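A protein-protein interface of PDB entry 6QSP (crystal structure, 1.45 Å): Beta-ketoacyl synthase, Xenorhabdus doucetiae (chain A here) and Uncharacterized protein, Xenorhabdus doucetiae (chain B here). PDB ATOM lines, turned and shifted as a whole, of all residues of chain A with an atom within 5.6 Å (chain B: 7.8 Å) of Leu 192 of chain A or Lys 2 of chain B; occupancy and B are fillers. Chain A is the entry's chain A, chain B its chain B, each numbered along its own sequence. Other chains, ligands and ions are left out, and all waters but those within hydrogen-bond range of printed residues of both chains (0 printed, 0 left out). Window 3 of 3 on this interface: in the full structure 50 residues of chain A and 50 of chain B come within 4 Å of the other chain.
Leu 192 of chain A touches just one residue of chain B: Lys 2.
Lys 2 of chain B touches one residue of chain A.
No residue of chain B comes within 4 Å of Gly 191 of chain A.
Of the printed residues of chain A, Phe 144 of chain B touches Pro 166 (3.8 Å).
Of the printed residues of chain B, Met 190 of chain A touches Leu 147 and Thr 148.
Printed residues of chain A within 4 Å of Thr 148 of chain B: Leu 187 (3.7 Å) and Met 190 (3.9 Å).
Ser 238 of chain B touches none of the printed residues of chain A.
Leu 3 of chain B touches none of the printed residues of chain A.
The nearest residue of chain B that does not touch Leu 192 of chain A is Phe 144 of chain B (4.1 Å).
Pro 166 of chain A touches Phe 144 of chain B.
CD2 of Leu 187 of chain A touches CG2 of Thr 148 of chain B (3.7 Å).
Met 190 of chain A touches Leu 147 of chain B.
SD of Met 190 of chain A touches CA of Thr 148 of chain B (3.9 Å).
O of Lys 2 of chain B touches CD2 of Leu 192 of chain A (3.5 Å).
Of the 15 printed residues of chain B, 4 touch a printed residue of chain A.
Hydrophobic or aromatic side chains of chain B within 4 Å of the printed part of chain A: Phe 144 and Leu 147.
Along chain B the printed residues that touch a printed residue of chain A span positions 2 to 148.
Of the 10 printed residues of chain A, 4 touch a printed residue of chain B.
Printed residues of chain A that touch a printed residue of chain B: Pro 166, Leu 187, Met 190 and Leu 192.
Among the printed residues, no Asp or Glu carboxylate lies within 4 Å of a Lys or Arg side-chain nitrogen of the other chain.
NH1 of Arg 109 of chain A sits at hydrogen-bond distance from O of Leu 192 of chain A (3.3 Å).
The backbone carbonyl oxygen (O) of Leu 187 of chain A is in hydrogen-bond range of the backbone NH (N) of Leu 192 of chain A (3.1 Å).
The backbone carbonyl oxygen of Leu 187 of chain A lies within hydrogen-bond range of the backbone NH of Val 193 of chain A.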
ATOM      1  N   GLU A 108      -4.386 -18.355  -9.773  1.00  0.00           N
ATOM      2  CA  GLU A 108      -3.502 -18.738 -10.908  1.00  0.00           C
ATOM      3  C   GLU A 108      -2.940 -20.153 -10.688  1.00  0.00           C
ATOM      4  O   GLU A 108      -2.472 -20.756 -11.677  1.00  0.00           O
ATOM      5  CB  GLU A 108      -2.392 -17.692 -11.068  1.00  0.00           C
ATOM      6  CG  GLU A 108      -2.899 -16.254 -11.069  1.00  0.00           C
ATOM      7  CD  GLU A 108      -3.058 -15.585  -9.706  1.00  0.00           C
ATOM      8  OE1 GLU A 108      -2.839 -16.262  -8.665  1.00  0.00           O
ATOM      9  OE2 GLU A 108      -3.407 -14.379  -9.679  1.00  0.00           O
ATOM     10  N   ARG A 109      -2.951 -20.666  -9.449  1.00  0.00           N
ATOM     11  CA  ARG A 109      -2.266 -21.940  -9.075  1.00  0.00           C
ATOM     12  C   ARG A 109      -3.305 -23.024  -8.746  1.00  0.00           C
ATOM     13  O   ARG A 109      -2.998 -23.972  -7.988  1.00  0.00           O
ATOM     14  CB  ARG A 109      -1.246 -21.653  -7.968  1.00  0.00           C
ATOM     15  CG  ARG A 109      -0.089 -20.783  -8.447  1.00  0.00           C
ATOM     16  CD  ARG A 109       1.184 -20.892  -7.628  1.00  0.00           C
ATOM     17  NE  ARG A 109       1.630 -22.271  -7.455  1.00  0.00           N
ATOM     18  CZ  ARG A 109       2.386 -22.966  -8.306  1.00  0.00           C
ATOM     19  NH1 ARG A 109       2.816 -22.435  -9.440  1.00  0.00           N
ATOM     20  NH2 ARG A 109       2.715 -24.210  -8.010  1.00  0.00           N
ATOM     21  N   PRO A 166      -4.693 -23.612 -15.647  1.00  0.00           N
ATOM     22  CA  PRO A 166      -5.141 -24.426 -16.776  1.00  0.00           C
ATOM     23  C   PRO A 166      -6.599 -24.847 -16.586  1.00  0.00           C
ATOM     24  O   PRO A 166      -6.992 -25.222 -15.491  1.00  0.00           O
ATOM     25  CB  PRO A 166      -4.201 -25.635 -16.752  1.00  0.00           C
ATOM     26  CG  PRO A 166      -2.947 -25.105 -16.086  1.00  0.00           C
ATOM     27  CD  PRO A 166      -3.469 -24.148 -15.032  1.00  0.00           C
ATOM     28  N   LEU A 187      -0.365 -31.900 -13.660  1.00  0.00           N
ATOM     29  CA  LEU A 187      -0.166 -30.424 -13.596  1.00  0.00           C
ATOM     30  C   LEU A 187       0.327 -30.026 -12.196  1.00  0.00           C
ATOM     31  O   LEU A 187       1.127 -29.074 -12.099  1.00  0.00           O
ATOM     32  CB  LEU A 187      -1.471 -29.719 -13.955  1.00  0.00           C
ATOM     33  CG  LEU A 187      -1.877 -29.827 -15.421  1.00  0.00           C
ATOM     34  CD1 LEU A 187      -3.306 -29.349 -15.608  1.00  0.00           C
ATOM     35  CD2 LEU A 187      -0.935 -29.036 -16.315  1.00  0.00           C
ATOM     36  N   ILE A 188      -0.107 -30.741 -11.153  1.00  0.00           N
ATOM     37  CA  ILE A 188       0.376 -30.508  -9.761  1.00  0.00           C
ATOM     38  C   ILE A 188       1.820 -31.035  -9.668  1.00  0.00           C
ATOM     39  O   ILE A 188       2.682 -30.295  -9.194  1.00  0.00           O
ATOM     40  CB  ILE A 188      -0.545 -31.130  -8.688  1.00  0.00           C
ATOM     41  CG1 ILE A 188      -1.980 -30.604  -8.788  1.00  0.00           C
ATOM     42  CG2 ILE A 188       0.055 -30.906  -7.307  1.00  0.00           C
ATOM     43  CD1 ILE A 188      -2.971 -31.406  -7.990  1.00  0.00           C
ATOM     44  N   MET A 190       4.027 -31.287 -11.924  1.00  0.00           N
ATOM     45  CA  MET A 190       4.867 -30.393 -12.767  1.00  0.00           C
ATOM     46  C   MET A 190       5.207 -29.097 -12.024  1.00  0.00           C
ATOM     47  O   MET A 190       6.167 -28.440 -12.443  1.00  0.00           O
ATOM     48  CB  MET A 190       4.138 -30.026 -14.060  1.00  0.00           C
ATOM     49  CG  MET A 190       4.132 -31.150 -15.050  1.00  0.00           C
ATOM     50  SD  MET A 190       2.835 -30.970 -16.266  1.00  0.00           S
ATOM     51  CE  MET A 190       3.596 -29.816 -17.405  1.00  0.00           C
ATOM     52  N   GLY A 191       4.419 -28.729 -11.008  1.00  0.00           N
ATOM     53  CA  GLY A 191       4.575 -27.465 -10.266  1.00  0.00           C
ATOM     54  C   GLY A 191       3.835 -26.300 -10.901  1.00  0.00           C
ATOM     55  O   GLY A 191       4.028 -25.165 -10.421  1.00  0.00           O
ATOM     56  N   LEU A 192       2.983 -26.541 -11.907  1.00  0.00           N
ATOM     57  CA  LEU A 192       2.220 -25.447 -12.578  1.00  0.00           C
ATOM     58  C   LEU A 192       1.092 -24.967 -11.662  1.00  0.00           C
ATOM     59  O   LEU A 192       0.750 -23.768 -11.700  1.00  0.00           O
ATOM     60  CB  LEU A 192       1.661 -25.939 -13.916  1.00  0.00           C
ATOM     61  CG  LEU A 192       2.637 -25.902 -15.089  1.00  0.00           C
ATOM     62  CD1 LEU A 192       2.026 -26.565 -16.309  1.00  0.00           C
ATOM     63  CD2 LEU A 192       3.054 -24.474 -15.416  1.00  0.00           C
ATOM     64  N   VAL A 193       0.523 -25.881 -10.882  1.00  0.00           N
ATOM     65  CA  VAL A 193      -0.572 -25.586  -9.912  1.00  0.00           C
ATOM     66  C   VAL A 193      -0.291 -26.362  -8.618  1.00  0.00           C
ATOM     67  O   VAL A 193       0.512 -27.324  -8.642  1.00  0.00           O
ATOM     68  CB  VAL A 193      -1.948 -25.936 -10.520  1.00  0.00           C
ATOM     69  CG1 VAL A 193      -2.271 -25.077 -11.733  1.00  0.00           C
ATOM     70  CG2 VAL A 193      -2.052 -27.413 -10.855  1.00  0.00           C
ATOM     71  N   ASP A 194      -0.932 -25.952  -7.525  1.00  0.00           N
ATOM     72  CA  ASP A 194      -0.844 -26.623  -6.204  1.00  0.00           C
ATOM     73  C   ASP A 194      -2.055 -27.526  -5.964  1.00  0.00           C
ATOM     74  O   ASP A 194      -1.951 -28.461  -5.141  1.00  0.00           O
ATOM     75  CB  ASP A 194      -0.727 -25.580  -5.100  1.00  0.00           C
ATOM     76  CG  ASP A 194       0.497 -24.716  -5.294  1.00  0.00           C
ATOM     77  OD1 ASP A 194       1.566 -25.305  -5.500  1.00  0.00           O
ATOM     78  OD2 ASP A 194       0.355 -23.467  -5.282  1.00  0.00           O
ATOM     79  N   LYS B   2       2.574 -20.514 -17.519  1.00  0.00           N
ATOM     80  CA  LYS B   2       3.696 -20.399 -18.475  1.00  0.00           C
ATOM     81  C   LYS B   2       4.181 -21.773 -18.936  1.00  0.00           C
ATOM     82  O   LYS B   2       4.307 -22.694 -18.149  1.00  0.00           O
ATOM     83  CB  LYS B   2       4.889 -19.714 -17.814  1.00  0.00           C
ATOM     84  CG  LYS B   2       6.163 -19.741 -18.639  1.00  0.00           C
ATOM     85  CD  LYS B   2       7.065 -18.611 -18.263  1.00  0.00           C
ATOM     86  CE  LYS B   2       8.384 -18.587 -18.996  1.00  0.00           C
ATOM     87  NZ  LYS B   2       9.265 -17.544 -18.425  1.00  0.00           N
ATOM     88  N   LEU B   3       4.527 -21.841 -20.215  1.00  0.00           N
ATOM     89  CA  LEU B   3       5.082 -23.102 -20.740  1.00  0.00           C
ATOM     90  C   LEU B   3       6.233 -22.827 -21.706  1.00  0.00           C
ATOM     91  O   LEU B   3       6.338 -21.747 -22.213  1.00  0.00           O
ATOM     92  CB  LEU B   3       3.981 -23.924 -21.391  1.00  0.00           C
ATOM     93  CG  LEU B   3       3.230 -23.231 -22.515  1.00  0.00           C
ATOM     94  CD1 LEU B   3       4.000 -23.356 -23.815  1.00  0.00           C
ATOM     95  CD2 LEU B   3       1.843 -23.820 -22.670  1.00  0.00           C
ATOM     96  N   THR B   4       7.122 -23.794 -21.798  1.00  0.00           N
ATOM     97  CA  THR B   4       8.254 -23.753 -22.750  1.00  0.00           C
ATOM     98  C   THR B   4       8.298 -25.100 -23.457  1.00  0.00           C
ATOM     99  O   THR B   4       8.052 -26.142 -22.796  1.00  0.00           O
ATOM    100  CB  THR B   4       9.574 -23.374 -22.062  1.00  0.00           C
ATOM    101  OG1 THR B   4      10.099 -24.530 -21.414  1.00  0.00           O
ATOM    102  CG2 THR B   4       9.410 -22.248 -21.067  1.00  0.00           C
ATOM    103  N   LEU B 143      -2.215 -27.447 -25.342  1.00  0.00           N
ATOM    104  CA  LEU B 143      -0.741 -27.490 -25.176  1.00  0.00           C
ATOM    105  C   LEU B 143      -0.401 -27.908 -23.742  1.00  0.00           C
ATOM    106  O   LEU B 143       0.605 -28.598 -23.574  1.00  0.00           O
ATOM    107  CB  LEU B 143      -0.139 -26.135 -25.558  1.00  0.00           C
ATOM    108  CG  LEU B 143      -0.162 -25.818 -27.054  1.00  0.00           C
ATOM    109  CD1 LEU B 143       0.330 -24.404 -27.313  1.00  0.00           C
ATOM    110  CD2 LEU B 143       0.663 -26.819 -27.848  1.00  0.00           C
ATOM    111  N   PHE B 144      -1.221 -27.563 -22.743  1.00  0.00           N
ATOM    112  CA  PHE B 144      -0.975 -28.017 -21.349  1.00  0.00           C
ATOM    113  C   PHE B 144      -1.122 -29.540 -21.284  1.00  0.00           C
ATOM    114  O   PHE B 144      -0.342 -30.175 -20.572  1.00  0.00           O
ATOM    115  CB  PHE B 144      -1.897 -27.365 -20.316  1.00  0.00           C
ATOM    116  CG  PHE B 144      -1.614 -25.924 -20.007  1.00  0.00           C
ATOM    117  CD1 PHE B 144      -0.390 -25.539 -19.480  1.00  0.00           C
ATOM    118  CD2 PHE B 144      -2.620 -24.974 -20.119  1.00  0.00           C
ATOM    119  CE1 PHE B 144      -0.142 -24.212 -19.169  1.00  0.00           C
ATOM    120  CE2 PHE B 144      -2.378 -23.647 -19.790  1.00  0.00           C
ATOM    121  CZ  PHE B 144      -1.140 -23.274 -19.315  1.00  0.00           C
ATOM    122  N   LEU B 147       1.992 -30.993 -22.671  1.00  0.00           N
ATOM    123  CA  LEU B 147       3.107 -30.816 -21.706  1.00  0.00           C
ATOM    124  C   LEU B 147       2.999 -31.847 -20.577  1.00  0.00           C
ATOM    125  O   LEU B 147       4.067 -32.305 -20.111  1.00  0.00           O
ATOM    126  CB  LEU B 147       3.088 -29.382 -21.183  1.00  0.00           C
ATOM    127  CG  LEU B 147       3.638 -28.359 -22.171  1.00  0.00           C
ATOM    128  CD1 LEU B 147       3.196 -26.962 -21.797  1.00  0.00           C
ATOM    129  CD2 LEU B 147       5.154 -28.430 -22.245  1.00  0.00           C
ATOM    130  N   THR B 148       1.790 -32.232 -20.146  1.00  0.00           N
ATOM    131  CA  THR B 148       1.642 -33.287 -19.106  1.00  0.00           C
ATOM    132  C   THR B 148       2.239 -34.588 -19.648  1.00  0.00           C
ATOM    133  O   THR B 148       2.821 -35.334 -18.855  1.00  0.00           O
ATOM    134  CB  THR B 148       0.207 -33.519 -18.603  1.00  0.00           C
ATOM    135  OG1 THR B 148      -0.604 -34.080 -19.641  1.00  0.00           O
ATOM    136  CG2 THR B 148      -0.414 -32.279 -17.994  1.00  0.00           C
ATOM    137  N   LEU B 195      10.644 -22.090 -27.538  1.00  0.00           N
ATOM    138  CA  LEU B 195       9.467 -21.196 -27.441  1.00  0.00           C
ATOM    139  C   LEU B 195       9.019 -21.152 -25.984  1.00  0.00           C
ATOM    140  O   LEU B 195       9.068 -22.190 -25.309  1.00  0.00           O
ATOM    141  CB  LEU B 195       8.330 -21.717 -28.323  1.00  0.00           C
ATOM    142  CG  LEU B 195       8.568 -21.667 -29.828  1.00  0.00           C
ATOM    143  CD1 LEU B 195       7.460 -22.407 -30.554  1.00  0.00           C
ATOM    144  CD2 LEU B 195       8.675 -20.235 -30.331  1.00  0.00           C
ATOM    145  N   SER B 196       8.593 -19.981 -25.534  1.00  0.00           N
ATOM    146  CA  SER B 196       7.893 -19.798 -24.244  1.00  0.00           C
ATOM    147  C   SER B 196       6.557 -19.105 -24.516  1.00  0.00           C
ATOM    148  O   SER B 196       6.439 -18.328 -25.485  1.00  0.00           O
ATOM    149  CB  SER B 196       8.738 -19.044 -23.251  1.00  0.00           C
ATOM    150  OG  SER B 196       8.845 -17.685 -23.628  1.00  0.00           O
ATOM    151  N   CYS B 197       5.579 -19.398 -23.677  1.00  0.00           N
ATOM    152  CA  CYS B 197       4.237 -18.803 -23.762  1.00  0.00           C
ATOM    153  C   CYS B 197       3.755 -18.467 -22.354  1.00  0.00           C
ATOM    154  O   CYS B 197       3.840 -19.345 -21.473  1.00  0.00           O
ATOM    155  CB  CYS B 197       3.280 -19.753 -24.465  1.00  0.00           C
ATOM    156  SG  CYS B 197       1.672 -18.995 -24.791  1.00  0.00           S
ATOM    157  N   THR B 198       3.270 -17.241 -22.172  1.00  0.00           N
ATOM    158  CA  THR B 198       2.630 -16.765 -20.921  1.00  0.00           C
ATOM    159  C   THR B 198       1.227 -16.233 -21.236  1.00  0.00           C
ATOM    160  O   THR B 198       1.055 -15.531 -22.245  1.00  0.00           O
ATOM    161  CB  THR B 198       3.504 -15.705 -20.243  1.00  0.00           C
ATOM    162  OG1 THR B 198       3.527 -14.591 -21.130  1.00  0.00           O
ATOM    163  CG2 THR B 198       4.918 -16.169 -19.966  1.00  0.00           C
ATOM    164  N   LYS B 199       0.257 -16.563 -20.390  1.00  0.00           N
ATOM    165  CA  LYS B 199      -1.159 -16.134 -20.541  1.00  0.00           C
ATOM    166  C   LYS B 199      -1.369 -14.777 -19.854  1.00  0.00           C
ATOM    167  O   LYS B 199      -0.767 -14.560 -18.792  1.00  0.00           O
ATOM    168  CB  LYS B 199      -2.068 -17.191 -19.921  1.00  0.00           C
ATOM    169  CG  LYS B 199      -3.558 -16.938 -20.061  1.00  0.00           C
ATOM    170  CD  LYS B 199      -4.359 -17.946 -19.292  1.00  0.00           C
ATOM    171  CE  LYS B 199      -5.830 -17.619 -19.229  1.00  0.00           C
ATOM    172  NZ  LYS B 199      -6.465 -18.324 -18.095  1.00  0.00           N
ATOM    173  N   TRP B 235      -2.237 -14.971 -25.233  1.00  0.00           N
ATOM    174  CA  TRP B 235      -1.116 -15.905 -25.010  1.00  0.00           C
ATOM    175  C   TRP B 235       0.101 -15.297 -25.700  1.00  0.00           C
ATOM    176  O   TRP B 235       0.080 -15.154 -26.937  1.00  0.00           O
ATOM    177  CB  TRP B 235      -1.501 -17.282 -25.540  1.00  0.00           C
ATOM    178  CG  TRP B 235      -2.746 -17.834 -24.912  1.00  0.00           C
ATOM    179  CD1 TRP B 235      -4.040 -17.592 -25.279  1.00  0.00           C
ATOM    180  CD2 TRP B 235      -2.811 -18.741 -23.801  1.00  0.00           C
ATOM    181  NE1 TRP B 235      -4.900 -18.303 -24.487  1.00  0.00           N
ATOM    182  CE2 TRP B 235      -4.176 -19.018 -23.570  1.00  0.00           C
ATOM    183  CE3 TRP B 235      -1.852 -19.382 -23.013  1.00  0.00           C
ATOM    184  CZ2 TRP B 235      -4.596 -19.890 -22.572  1.00  0.00           C
ATOM    185  CZ3 TRP B 235      -2.268 -20.256 -22.036  1.00  0.00           C
ATOM    186  CH2 TRP B 235      -3.624 -20.499 -21.813  1.00  0.00           C
ATOM    187  N   ASN B 236       1.061 -14.867 -24.886  1.00  0.00           N
ATOM    188  CA  ASN B 236       2.263 -14.109 -25.312  1.00  0.00           C
ATOM    189  C   ASN B 236       3.386 -15.101 -25.602  1.00  0.00           C
ATOM    190  O   ASN B 236       3.926 -15.673 -24.644  1.00  0.00           O
ATOM    191  CB  ASN B 236       2.658 -13.090 -24.246  1.00  0.00           C
ATOM    192  CG  ASN B 236       1.565 -12.078 -23.993  1.00  0.00           C
ATOM    193  OD1 ASN B 236       0.938 -11.593 -24.927  1.00  0.00           O
ATOM    194  ND2 ASN B 236       1.350 -11.733 -22.737  1.00  0.00           N
ATOM    195  N   SER B 238       7.145 -16.079 -27.173  1.00  0.00           N
ATOM    196  CA  SER B 238       8.476 -15.488 -27.436  1.00  0.00           C
ATOM    197  C   SER B 238       9.466 -16.562 -27.907  1.00  0.00           C
ATOM    198  O   SER B 238       9.385 -17.715 -27.430  1.00  0.00           O
ATOM    199  CB  SER B 238       8.957 -14.708 -26.243  1.00  0.00           C
ATOM    200  OG  SER B 238       9.107 -15.544 -25.116  1.00  0.00           O
